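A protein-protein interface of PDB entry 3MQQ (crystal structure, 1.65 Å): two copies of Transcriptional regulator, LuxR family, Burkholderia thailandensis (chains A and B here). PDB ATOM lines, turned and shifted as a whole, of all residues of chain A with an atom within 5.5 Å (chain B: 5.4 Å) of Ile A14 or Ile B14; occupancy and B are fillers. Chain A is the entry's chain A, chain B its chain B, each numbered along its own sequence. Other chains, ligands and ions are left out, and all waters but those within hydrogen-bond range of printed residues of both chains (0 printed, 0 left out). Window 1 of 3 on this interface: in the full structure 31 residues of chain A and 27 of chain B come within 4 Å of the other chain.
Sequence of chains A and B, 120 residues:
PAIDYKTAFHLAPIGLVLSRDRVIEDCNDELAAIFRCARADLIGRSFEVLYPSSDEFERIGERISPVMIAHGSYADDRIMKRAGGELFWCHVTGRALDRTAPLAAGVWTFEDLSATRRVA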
ATOM      1  N   ALA A  12      -8.411  14.431 -17.596  1.00  0.00           N
ATOM      2  CA  ALA A  12      -7.935  13.084 -17.330  1.00  0.00           C
ATOM      3  C   ALA A  12      -7.780  12.283 -18.612  1.00  0.00           C
ATOM      4  O   ALA A  12      -8.631  12.365 -19.489  1.00  0.00           O
ATOM      5  CB  ALA A  12      -8.857  12.353 -16.348  1.00  0.00           C
ATOM      6  N   PRO A  13      -6.701  11.494 -18.701  1.00  0.00           N
ATOM      7  CA  PRO A  13      -6.380  10.683 -19.874  1.00  0.00           C
ATOM      8  C   PRO A  13      -7.206   9.411 -20.022  1.00  0.00           C
ATOM      9  O   PRO A  13      -6.945   8.613 -20.925  1.00  0.00           O
ATOM     10  CB  PRO A  13      -4.901  10.327 -19.657  1.00  0.00           C
ATOM     11  CG  PRO A  13      -4.737  10.362 -18.197  1.00  0.00           C
ATOM     12  CD  PRO A  13      -5.609  11.470 -17.712  1.00  0.00           C
ATOM     13  N   ILE A  14      -8.152   9.202 -19.119  1.00  0.00           N
ATOM     14  CA  ILE A  14      -9.112   8.109 -19.258  1.00  0.00           C
ATOM     15  C   ILE A  14     -10.520   8.644 -19.271  1.00  0.00           C
ATOM     16  O   ILE A  14     -10.762   9.741 -18.768  1.00  0.00           O
ATOM     17  CB  ILE A  14      -8.949   7.040 -18.150  1.00  0.00           C
ATOM     18  CG1 ILE A  14      -9.205   7.602 -16.759  1.00  0.00           C
ATOM     19  CG2 ILE A  14      -7.567   6.360 -18.260  1.00  0.00           C
ATOM     20  CD1 ILE A  14      -9.141   6.535 -15.691  1.00  0.00           C
ATOM     21  N   GLY A  15     -11.457   7.897 -19.845  1.00  0.00           N
ATOM     22  CA  GLY A  15     -12.855   8.341 -19.789  1.00  0.00           C
ATOM     23  C   GLY A  15     -13.377   8.332 -18.357  1.00  0.00           C
ATOM     24  O   GLY A  15     -13.178   7.362 -17.635  1.00  0.00           O
ATOM     25  N   LEU A  16     -14.060   9.404 -17.954  1.00  0.00           N
ATOM     26  CA  LEU A  16     -14.617   9.459 -16.608  1.00  0.00           C
ATOM     27  C   LEU A  16     -16.094   9.811 -16.720  1.00  0.00           C
ATOM     28  O   LEU A  16     -16.492  10.615 -17.591  1.00  0.00           O
ATOM     29  CB  LEU A  16     -13.918  10.503 -15.762  1.00  0.00           C
ATOM     30  CG  LEU A  16     -12.451  10.287 -15.437  1.00  0.00           C
ATOM     31  CD1 LEU A  16     -12.001  11.538 -14.701  1.00  0.00           C
ATOM     32  CD2 LEU A  16     -12.274   9.025 -14.561  1.00  0.00           C
ATOM     33  N   ASN A  28     -16.138  13.395 -19.281  1.00  0.00           N
ATOM     34  CA  ASN A  28     -15.031  14.216 -19.772  1.00  0.00           C
ATOM     35  C   ASN A  28     -14.837  13.994 -21.262  1.00  0.00           C
ATOM     36  O   ASN A  28     -15.476  13.109 -21.856  1.00  0.00           O
ATOM     37  CB  ASN A  28     -13.751  13.990 -18.947  1.00  0.00           C
ATOM     38  CG  ASN A  28     -13.215  12.564 -19.065  1.00  0.00           C
ATOM     39  OD1 ASN A  28     -13.790  11.708 -19.751  1.00  0.00           O
ATOM     40  ND2 ASN A  28     -12.108  12.306 -18.385  1.00  0.00           N
ATOM     41  N   GLU A  30     -12.353  12.809 -22.805  1.00  0.00           N
ATOM     42  CA  GLU A  30     -11.753  11.499 -23.118  1.00  0.00           C
ATOM     43  C   GLU A  30     -12.804  10.428 -23.347  1.00  0.00           C
ATOM     44  O   GLU A  30     -12.621   9.542 -24.201  1.00  0.00           O
ATOM     45  CB  GLU A  30     -10.756  11.053 -22.043  1.00  0.00           C
ATOM     46  CG  GLU A  30      -9.830   9.889 -22.457  1.00  0.00           C
ATOM     47  CD  GLU A  30      -8.869  10.263 -23.598  1.00  0.00           C
ATOM     48  OE1 GLU A  30      -8.554  11.451 -23.768  1.00  0.00           O
ATOM     49  OE2 GLU A  30      -8.405   9.368 -24.327  1.00  0.00           O
ATOM     50  N   LEU A  31     -13.892  10.481 -22.591  1.00  0.00           N
ATOM     51  CA  LEU A  31     -14.955   9.479 -22.779  1.00  0.00           C
ATOM     52  C   LEU A  31     -15.545   9.662 -24.180  1.00  0.00           C
ATOM     53  O   LEU A  31     -15.767   8.686 -24.907  1.00  0.00           O
ATOM     54  CB  LEU A  31     -16.040   9.581 -21.704  1.00  0.00           C
ATOM     55  CG  LEU A  31     -17.100   8.476 -21.900  1.00  0.00           C
ATOM     56  CD1 LEU A  31     -16.556   7.116 -21.405  1.00  0.00           C
ATOM     57  CD2 LEU A  31     -18.414   8.828 -21.223  1.00  0.00           C
ATOM     58  N   ILE A  34     -13.054   8.212 -26.733  1.00  0.00           N
ATOM     59  CA  ILE A  34     -13.132   6.762 -26.829  1.00  0.00           C
ATOM     60  C   ILE A  34     -14.339   6.335 -27.650  1.00  0.00           C
ATOM     61  O   ILE A  34     -14.231   5.443 -28.515  1.00  0.00           O
ATOM     62  CB  ILE A  34     -13.237   6.136 -25.430  1.00  0.00           C
ATOM     63  CG1 ILE A  34     -11.941   6.385 -24.647  1.00  0.00           C
ATOM     64  CG2 ILE A  34     -13.558   4.671 -25.505  1.00  0.00           C
ATOM     65  CD1 ILE A  34     -12.047   6.050 -23.160  1.00  0.00           C
ATOM     66  N   THR A  93     -13.959   0.585 -14.548  1.00  0.00           N
ATOM     67  CA  THR A  93     -13.955   0.447 -13.096  1.00  0.00           C
ATOM     68  C   THR A  93     -15.037   1.369 -12.567  1.00  0.00           C
ATOM     69  O   THR A  93     -15.419   2.335 -13.215  1.00  0.00           O
ATOM     70  CB  THR A  93     -12.606   0.808 -12.406  1.00  0.00           C
ATOM     71  OG1 THR A  93     -12.448   2.225 -12.328  1.00  0.00           O
ATOM     72  CG2 THR A  93     -11.395   0.207 -13.132  1.00  0.00           C
ATOM     73  N   ARG A  95     -17.088   2.905  -8.699  1.00  0.00           N
ATOM     74  CA  ARG A  95     -17.360   2.860  -7.267  1.00  0.00           C
ATOM     75  C   ARG A  95     -18.654   3.598  -7.036  1.00  0.00           C
ATOM     76  O   ARG A  95     -18.780   4.764  -7.388  1.00  0.00           O
ATOM     77  CB  ARG A  95     -16.246   3.492  -6.419  1.00  0.00           C
ATOM     78  CG  ARG A  95     -16.651   3.406  -4.947  1.00  0.00           C
ATOM     79  CD  ARG A  95     -15.535   3.645  -3.997  1.00  0.00           C
ATOM     80  NE  ARG A  95     -14.727   2.453  -3.795  1.00  0.00           N
ATOM     81  CZ  ARG A  95     -13.397   2.447  -3.849  1.00  0.00           C
ATOM     82  NH1 ARG A  95     -12.711   1.324  -3.621  1.00  0.00           N
ATOM     83  NH2 ARG A  95     -12.749   3.571  -4.129  1.00  0.00           N
ATOM     84  N   THR A 109     -15.006   4.698 -14.657  1.00  0.00           N
ATOM     85  CA  THR A 109     -13.875   4.926 -15.569  1.00  0.00           C
ATOM     86  C   THR A 109     -13.907   3.995 -16.753  1.00  0.00           C
ATOM     87  O   THR A 109     -14.410   2.872 -16.658  1.00  0.00           O
ATOM     88  CB  THR A 109     -12.498   4.813 -14.859  1.00  0.00           C
ATOM     89  OG1 THR A 109     -12.137   3.417 -14.730  1.00  0.00           O
ATOM     90  CG2 THR A 109     -12.460   5.539 -13.509  1.00  0.00           C
ATOM     91  N   PHE A 110     -13.387   4.485 -17.888  1.00  0.00           N
ATOM     92  CA  PHE A 110     -13.371   3.749 -19.140  1.00  0.00           C
ATOM     93  C   PHE A 110     -12.017   3.916 -19.810  1.00  0.00           C
ATOM     94  O   PHE A 110     -11.528   5.021 -19.927  1.00  0.00           O
ATOM     95  CB  PHE A 110     -14.465   4.286 -20.087  1.00  0.00           C
ATOM     96  CG  PHE A 110     -15.853   4.095 -19.552  1.00  0.00           C
ATOM     97  CD1 PHE A 110     -16.619   2.995 -19.940  1.00  0.00           C
ATOM     98  CD2 PHE A 110     -16.379   4.997 -18.603  1.00  0.00           C
ATOM     99  CE1 PHE A 110     -17.902   2.805 -19.403  1.00  0.00           C
ATOM    100  CE2 PHE A 110     -17.649   4.799 -18.054  1.00  0.00           C
ATOM    101  CZ  PHE A 110     -18.411   3.717 -18.465  1.00  0.00           C
ATOM    102  N   GLU A 111     -11.416   2.804 -20.234  1.00  0.00           N
ATOM    103  CA  GLU A 111     -10.151   2.869 -20.943  1.00  0.00           C
ATOM    104  C   GLU A 111     -10.180   1.868 -22.081  1.00  0.00           C
ATOM    105  O   GLU A 111     -10.519   0.733 -21.879  1.00  0.00           O
ATOM    106  CB  GLU A 111      -8.974   2.578 -20.010  1.00  0.00           C
ATOM    107  CG  GLU A 111      -7.624   2.606 -20.736  1.00  0.00           C
ATOM    108  CD  GLU A 111      -6.449   2.660 -19.774  1.00  0.00           C
ATOM    109  OE1 GLU A 111      -6.631   2.406 -18.562  1.00  0.00           O
ATOM    110  OE2 GLU A 111      -5.325   2.962 -20.214  1.00  0.00           O
ATOM    111  N   ALA B  12     -13.029   7.763  -6.290  1.00  0.00           N
ATOM    112  CA  ALA B  12     -12.631   6.996  -7.483  1.00  0.00           C
ATOM    113  C   ALA B  12     -11.986   5.676  -7.142  1.00  0.00           C
ATOM    114  O   ALA B  12     -11.176   5.606  -6.252  1.00  0.00           O
ATOM    115  CB  ALA B  12     -11.686   7.824  -8.379  1.00  0.00           C
ATOM    116  N   PRO B  13     -12.331   4.611  -7.885  1.00  0.00           N
ATOM    117  CA  PRO B  13     -11.881   3.256  -7.613  1.00  0.00           C
ATOM    118  C   PRO B  13     -10.462   2.991  -8.088  1.00  0.00           C
ATOM    119  O   PRO B  13      -9.991   1.836  -8.030  1.00  0.00           O
ATOM    120  CB  PRO B  13     -12.854   2.400  -8.433  1.00  0.00           C
ATOM    121  CG  PRO B  13     -13.318   3.284  -9.520  1.00  0.00           C
ATOM    122  CD  PRO B  13     -13.306   4.686  -8.979  1.00  0.00           C
ATOM    123  N   ILE B  14      -9.839   4.022  -8.640  1.00  0.00           N
ATOM    124  CA  ILE B  14      -8.432   3.961  -9.044  1.00  0.00           C
ATOM    125  C   ILE B  14      -7.670   5.078  -8.345  1.00  0.00           C
ATOM    126  O   ILE B  14      -8.239   6.102  -7.948  1.00  0.00           O
ATOM    127  CB  ILE B  14      -8.231   4.103 -10.572  1.00  0.00           C
ATOM    128  CG1 ILE B  14      -8.772   5.448 -11.066  1.00  0.00           C
ATOM    129  CG2 ILE B  14      -8.845   2.914 -11.319  1.00  0.00           C
ATOM    130  CD1 ILE B  14      -8.478   5.718 -12.497  1.00  0.00           C
ATOM    131  N   GLY B  15      -6.372   4.881  -8.221  1.00  0.00           N
ATOM    132  CA  GLY B  15      -5.524   5.891  -7.614  1.00  0.00           C
ATOM    133  C   GLY B  15      -5.428   7.103  -8.510  1.00  0.00           C
ATOM    134  O   GLY B  15      -5.235   6.981  -9.721  1.00  0.00           O
ATOM    135  N   LEU B  16      -5.636   8.276  -7.926  1.00  0.00           N
ATOM    136  CA  LEU B  16      -5.510   9.525  -8.714  1.00  0.00           C
ATOM    137  C   LEU B  16      -4.530  10.462  -8.043  1.00  0.00           C
ATOM    138  O   LEU B  16      -4.439  10.537  -6.800  1.00  0.00           O
ATOM    139  CB  LEU B  16      -6.847  10.266  -8.824  1.00  0.00           C
ATOM    140  CG  LEU B  16      -7.971   9.527  -9.524  1.00  0.00           C
ATOM    141  CD1 LEU B  16      -9.244  10.338  -9.397  1.00  0.00           C
ATOM    142  CD2 LEU B  16      -7.616   9.284 -10.980  1.00  0.00           C
ATOM    143  N   ASN B  28      -5.862  10.599  -3.853  1.00  0.00           N
ATOM    144  CA  ASN B  28      -7.002  10.004  -3.188  1.00  0.00           C
ATOM    145  C   ASN B  28      -6.639   8.804  -2.304  1.00  0.00           C
ATOM    146  O   ASN B  28      -5.466   8.336  -2.290  1.00  0.00           O
ATOM    147  CB  ASN B  28      -8.134   9.663  -4.200  1.00  0.00           C
ATOM    148  CG  ASN B  28      -7.742   8.618  -5.229  1.00  0.00           C
ATOM    149  OD1 ASN B  28      -6.659   8.023  -5.188  1.00  0.00           O
ATOM    150  ND2 ASN B  28      -8.655   8.380  -6.168  1.00  0.00           N
ATOM    151  N   GLU B  30      -7.558   5.722  -2.676  1.00  0.00           N
ATOM    152  CA  GLU B  30      -7.161   4.540  -3.440  1.00  0.00           C
ATOM    153  C   GLU B  30      -5.660   4.501  -3.699  1.00  0.00           C
ATOM    154  O   GLU B  30      -5.050   3.405  -3.632  1.00  0.00           O
ATOM    155  CB  GLU B  30      -7.959   4.409  -4.748  1.00  0.00           C
ATOM    156  CG  GLU B  30      -7.726   3.087  -5.567  1.00  0.00           C
ATOM    157  CD  GLU B  30      -8.004   1.808  -4.798  1.00  0.00           C
ATOM    158  OE1 GLU B  30      -8.900   1.805  -3.937  1.00  0.00           O
ATOM    159  OE2 GLU B  30      -7.333   0.780  -5.089  1.00  0.00           O
ATOM    160  N   LEU B  31      -5.068   5.651  -4.024  1.00  0.00           N
ATOM    161  CA  LEU B  31      -3.599   5.698  -4.216  1.00  0.00           C
ATOM    162  C   LEU B  31      -2.875   5.257  -2.943  1.00  0.00           C
ATOM    163  O   LEU B  31      -1.924   4.449  -3.005  1.00  0.00           O
ATOM    164  CB  LEU B  31      -3.120   7.087  -4.645  1.00  0.00           C
ATOM    165  CG  LEU B  31      -1.622   6.997  -4.980  1.00  0.00           C
ATOM    166  CD1 LEU B  31      -1.382   6.383  -6.376  1.00  0.00           C
ATOM    167  CD2 LEU B  31      -0.930   8.343  -4.823  1.00  0.00           C
ATOM    168  N   ILE B  34      -3.130   1.495  -2.588  1.00  0.00           N
ATOM    169  CA  ILE B  34      -2.239   0.766  -3.487  1.00  0.00           C
ATOM    170  C   ILE B  34      -0.830   0.732  -2.902  1.00  0.00           C
ATOM    171  O   ILE B  34      -0.165  -0.322  -2.894  1.00  0.00           O
ATOM    172  CB  ILE B  34      -2.205   1.400  -4.896  1.00  0.00           C
ATOM    173  CG1 ILE B  34      -3.575   1.286  -5.594  1.00  0.00           C
ATOM    174  CG2 ILE B  34      -1.082   0.784  -5.738  1.00  0.00           C
ATOM    175  CD1 ILE B  34      -3.733   2.205  -6.820  1.00  0.00           C
ATOM    176  N   THR B  93      -1.526   6.063 -16.134  1.00  0.00           N
ATOM    177  CA  THR B  93      -1.838   6.971 -17.246  1.00  0.00           C
ATOM    178  C   THR B  93      -1.629   8.394 -16.791  1.00  0.00           C
ATOM    179  O   THR B  93      -1.724   8.694 -15.615  1.00  0.00           O
ATOM    180  CB  THR B  93      -3.269   6.799 -17.869  1.00  0.00           C
ATOM    181  OG1 THR B  93      -4.264   7.464 -17.083  1.00  0.00           O
ATOM    182  CG2 THR B  93      -3.658   5.331 -18.079  1.00  0.00           C
ATOM    183  N   THR B 109      -2.993   8.636 -13.144  1.00  0.00           N
ATOM    184  CA  THR B 109      -3.833   7.555 -12.615  1.00  0.00           C
ATOM    185  C   THR B 109      -2.969   6.348 -12.369  1.00  0.00           C
ATOM    186  O   THR B 109      -2.012   6.125 -13.086  1.00  0.00           O
ATOM    187  CB  THR B 109      -5.025   7.143 -13.557  1.00  0.00           C
ATOM    188  OG1 THR B 109      -4.524   6.406 -14.682  1.00  0.00           O
ATOM    189  CG2 THR B 109      -5.839   8.332 -14.059  1.00  0.00           C
ATOM    190  N   PHE B 110      -3.344   5.546 -11.368  1.00  0.00           N
ATOM    191  CA  PHE B 110      -2.586   4.343 -11.010  1.00  0.00           C
ATOM    192  C   PHE B 110      -3.587   3.227 -10.717  1.00  0.00           C
ATOM    193  O   PHE B 110      -4.535   3.456 -10.001  1.00  0.00           O
ATOM    194  CB  PHE B 110      -1.814   4.621  -9.712  1.00  0.00           C
ATOM    195  CG  PHE B 110      -0.774   5.689  -9.857  1.00  0.00           C
ATOM    196  CD1 PHE B 110       0.556   5.347 -10.014  1.00  0.00           C
ATOM    197  CD2 PHE B 110      -1.132   7.033  -9.860  1.00  0.00           C
ATOM    198  CE1 PHE B 110       1.523   6.345 -10.206  1.00  0.00           C
ATOM    199  CE2 PHE B 110      -0.157   8.023 -10.028  1.00  0.00           C
ATOM    200  CZ  PHE B 110       1.147   7.678 -10.195  1.00  0.00           C
ATOM    201  N   GLU B 111      -3.368   2.032 -11.259  1.00  0.00           N
ATOM    202  CA  GLU B 111      -4.229   0.946 -10.939  1.00  0.00           C
ATOM    203  C   GLU B 111      -3.376  -0.299 -10.679  1.00  0.00           C
ATOM    204  O   GLU B 111      -2.534  -0.634 -11.478  1.00  0.00           O
ATOM    205  CB  GLU B 111      -5.204   0.698 -12.098  1.00  0.00           C
ATOM    206  CG  GLU B 111      -6.104  -0.488 -11.854  1.00  0.00           C
ATOM    207  CD  GLU B 111      -7.054  -0.719 -12.989  1.00  0.00           C
ATOM    208  OE1 GLU B 111      -6.749  -0.286 -14.118  1.00  0.00           O
ATOM    209  OE2 GLU B 111      -8.112  -1.334 -12.758  1.00  0.00           O
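Ile A14 touches just these residues of chain B: Ile B14 and Thr B93.
Ile B14 touches two residues of chain A.
Of the printed residues of chain A, Glu B111 touches Thr A93.
Of the printed residues of chain B, Thr A93 touches Pro B13 (3.1 Å), Ile B14 (3.8 Å) and Glu B111 (3.6 Å).
Of the printed residues of chain B, Pro A13 touches Thr B93 (3.1 Å).
Of the printed residues of chain B, Arg A95 touches Ala B12 (3.3 Å), Pro B13 (3.6 Å) and Glu B30 (3.9 Å).
Of the printed residues of chain A, Ala B12 touches Arg A95 (3.3 Å).
Leu B16 touches none of the printed residues of chain A.
Glu A30 touches none of the printed residues of chain B.
The nearest printed residue of chain B that does not touch Thr A93 is Ala B12 (6.2 Å).
Of the 14 printed residues of chain A, 5 touch a printed residue of chain B.
Hydrophobic or aromatic side chains of chain A within 4 Å of the printed part of chain B: Pro A13 and Ile A14.
Of the 13 printed residues of chain B, 6 touch a printed residue of chain A.
Among the printed residues, pairs that only touch across the chains: Pro A13 with Thr B93 (3.1 Å), Ile A14 with Ile B14 (3.4 Å), Ile A14 with Thr B93 (3.7 Å), Thr A93 with Pro B13 (3.1 Å), Thr A93 with Ile B14 (3.8 Å), Thr A93 with Glu B111 (3.6 Å), Arg A95 with Pro B13 (3.6 Å) and Glu A111 with Thr B93 (3.6 Å).
NH1 of Arg A95 lies within salt-bridge range of OE1 of Glu B30, at 3.9 Å.
O of Ala B12 sits at hydrogen-bond distance from NH2 of Arg A95 (3.3 Å).
The side-chain hydroxyl of Thr A93 lies within hydrogen-bond range of the side-chain hydroxyl of Thr A109.
The backbone carbonyl oxygen of Ile B14 lies within hydrogen-bond range of the side-chain amide nitrogen of Asn B28, at 2.9 Å.
The side-chain hydroxyl (OG1) of Thr B93 sits at hydrogen-bond distance from the side-chain hydroxyl (OG1) of Thr B109 (2.6 Å).
O of Ile A14 lies within hydrogen-bond range of ND2 of Asn A28 (2.9 Å).
Pro A13 touches Thr B93, and with the chains exchanged Thr A93 touches Pro B13.
Ile B14 touches its own counterpart, Ile A14.
Ile A14 touches Thr B93, and with the chains exchanged Thr A93 touches Ile B14.
Thr A93 touches Glu B111, and with the chains exchanged Glu A111 touches Thr B93.
13 positions are printed for both chains.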
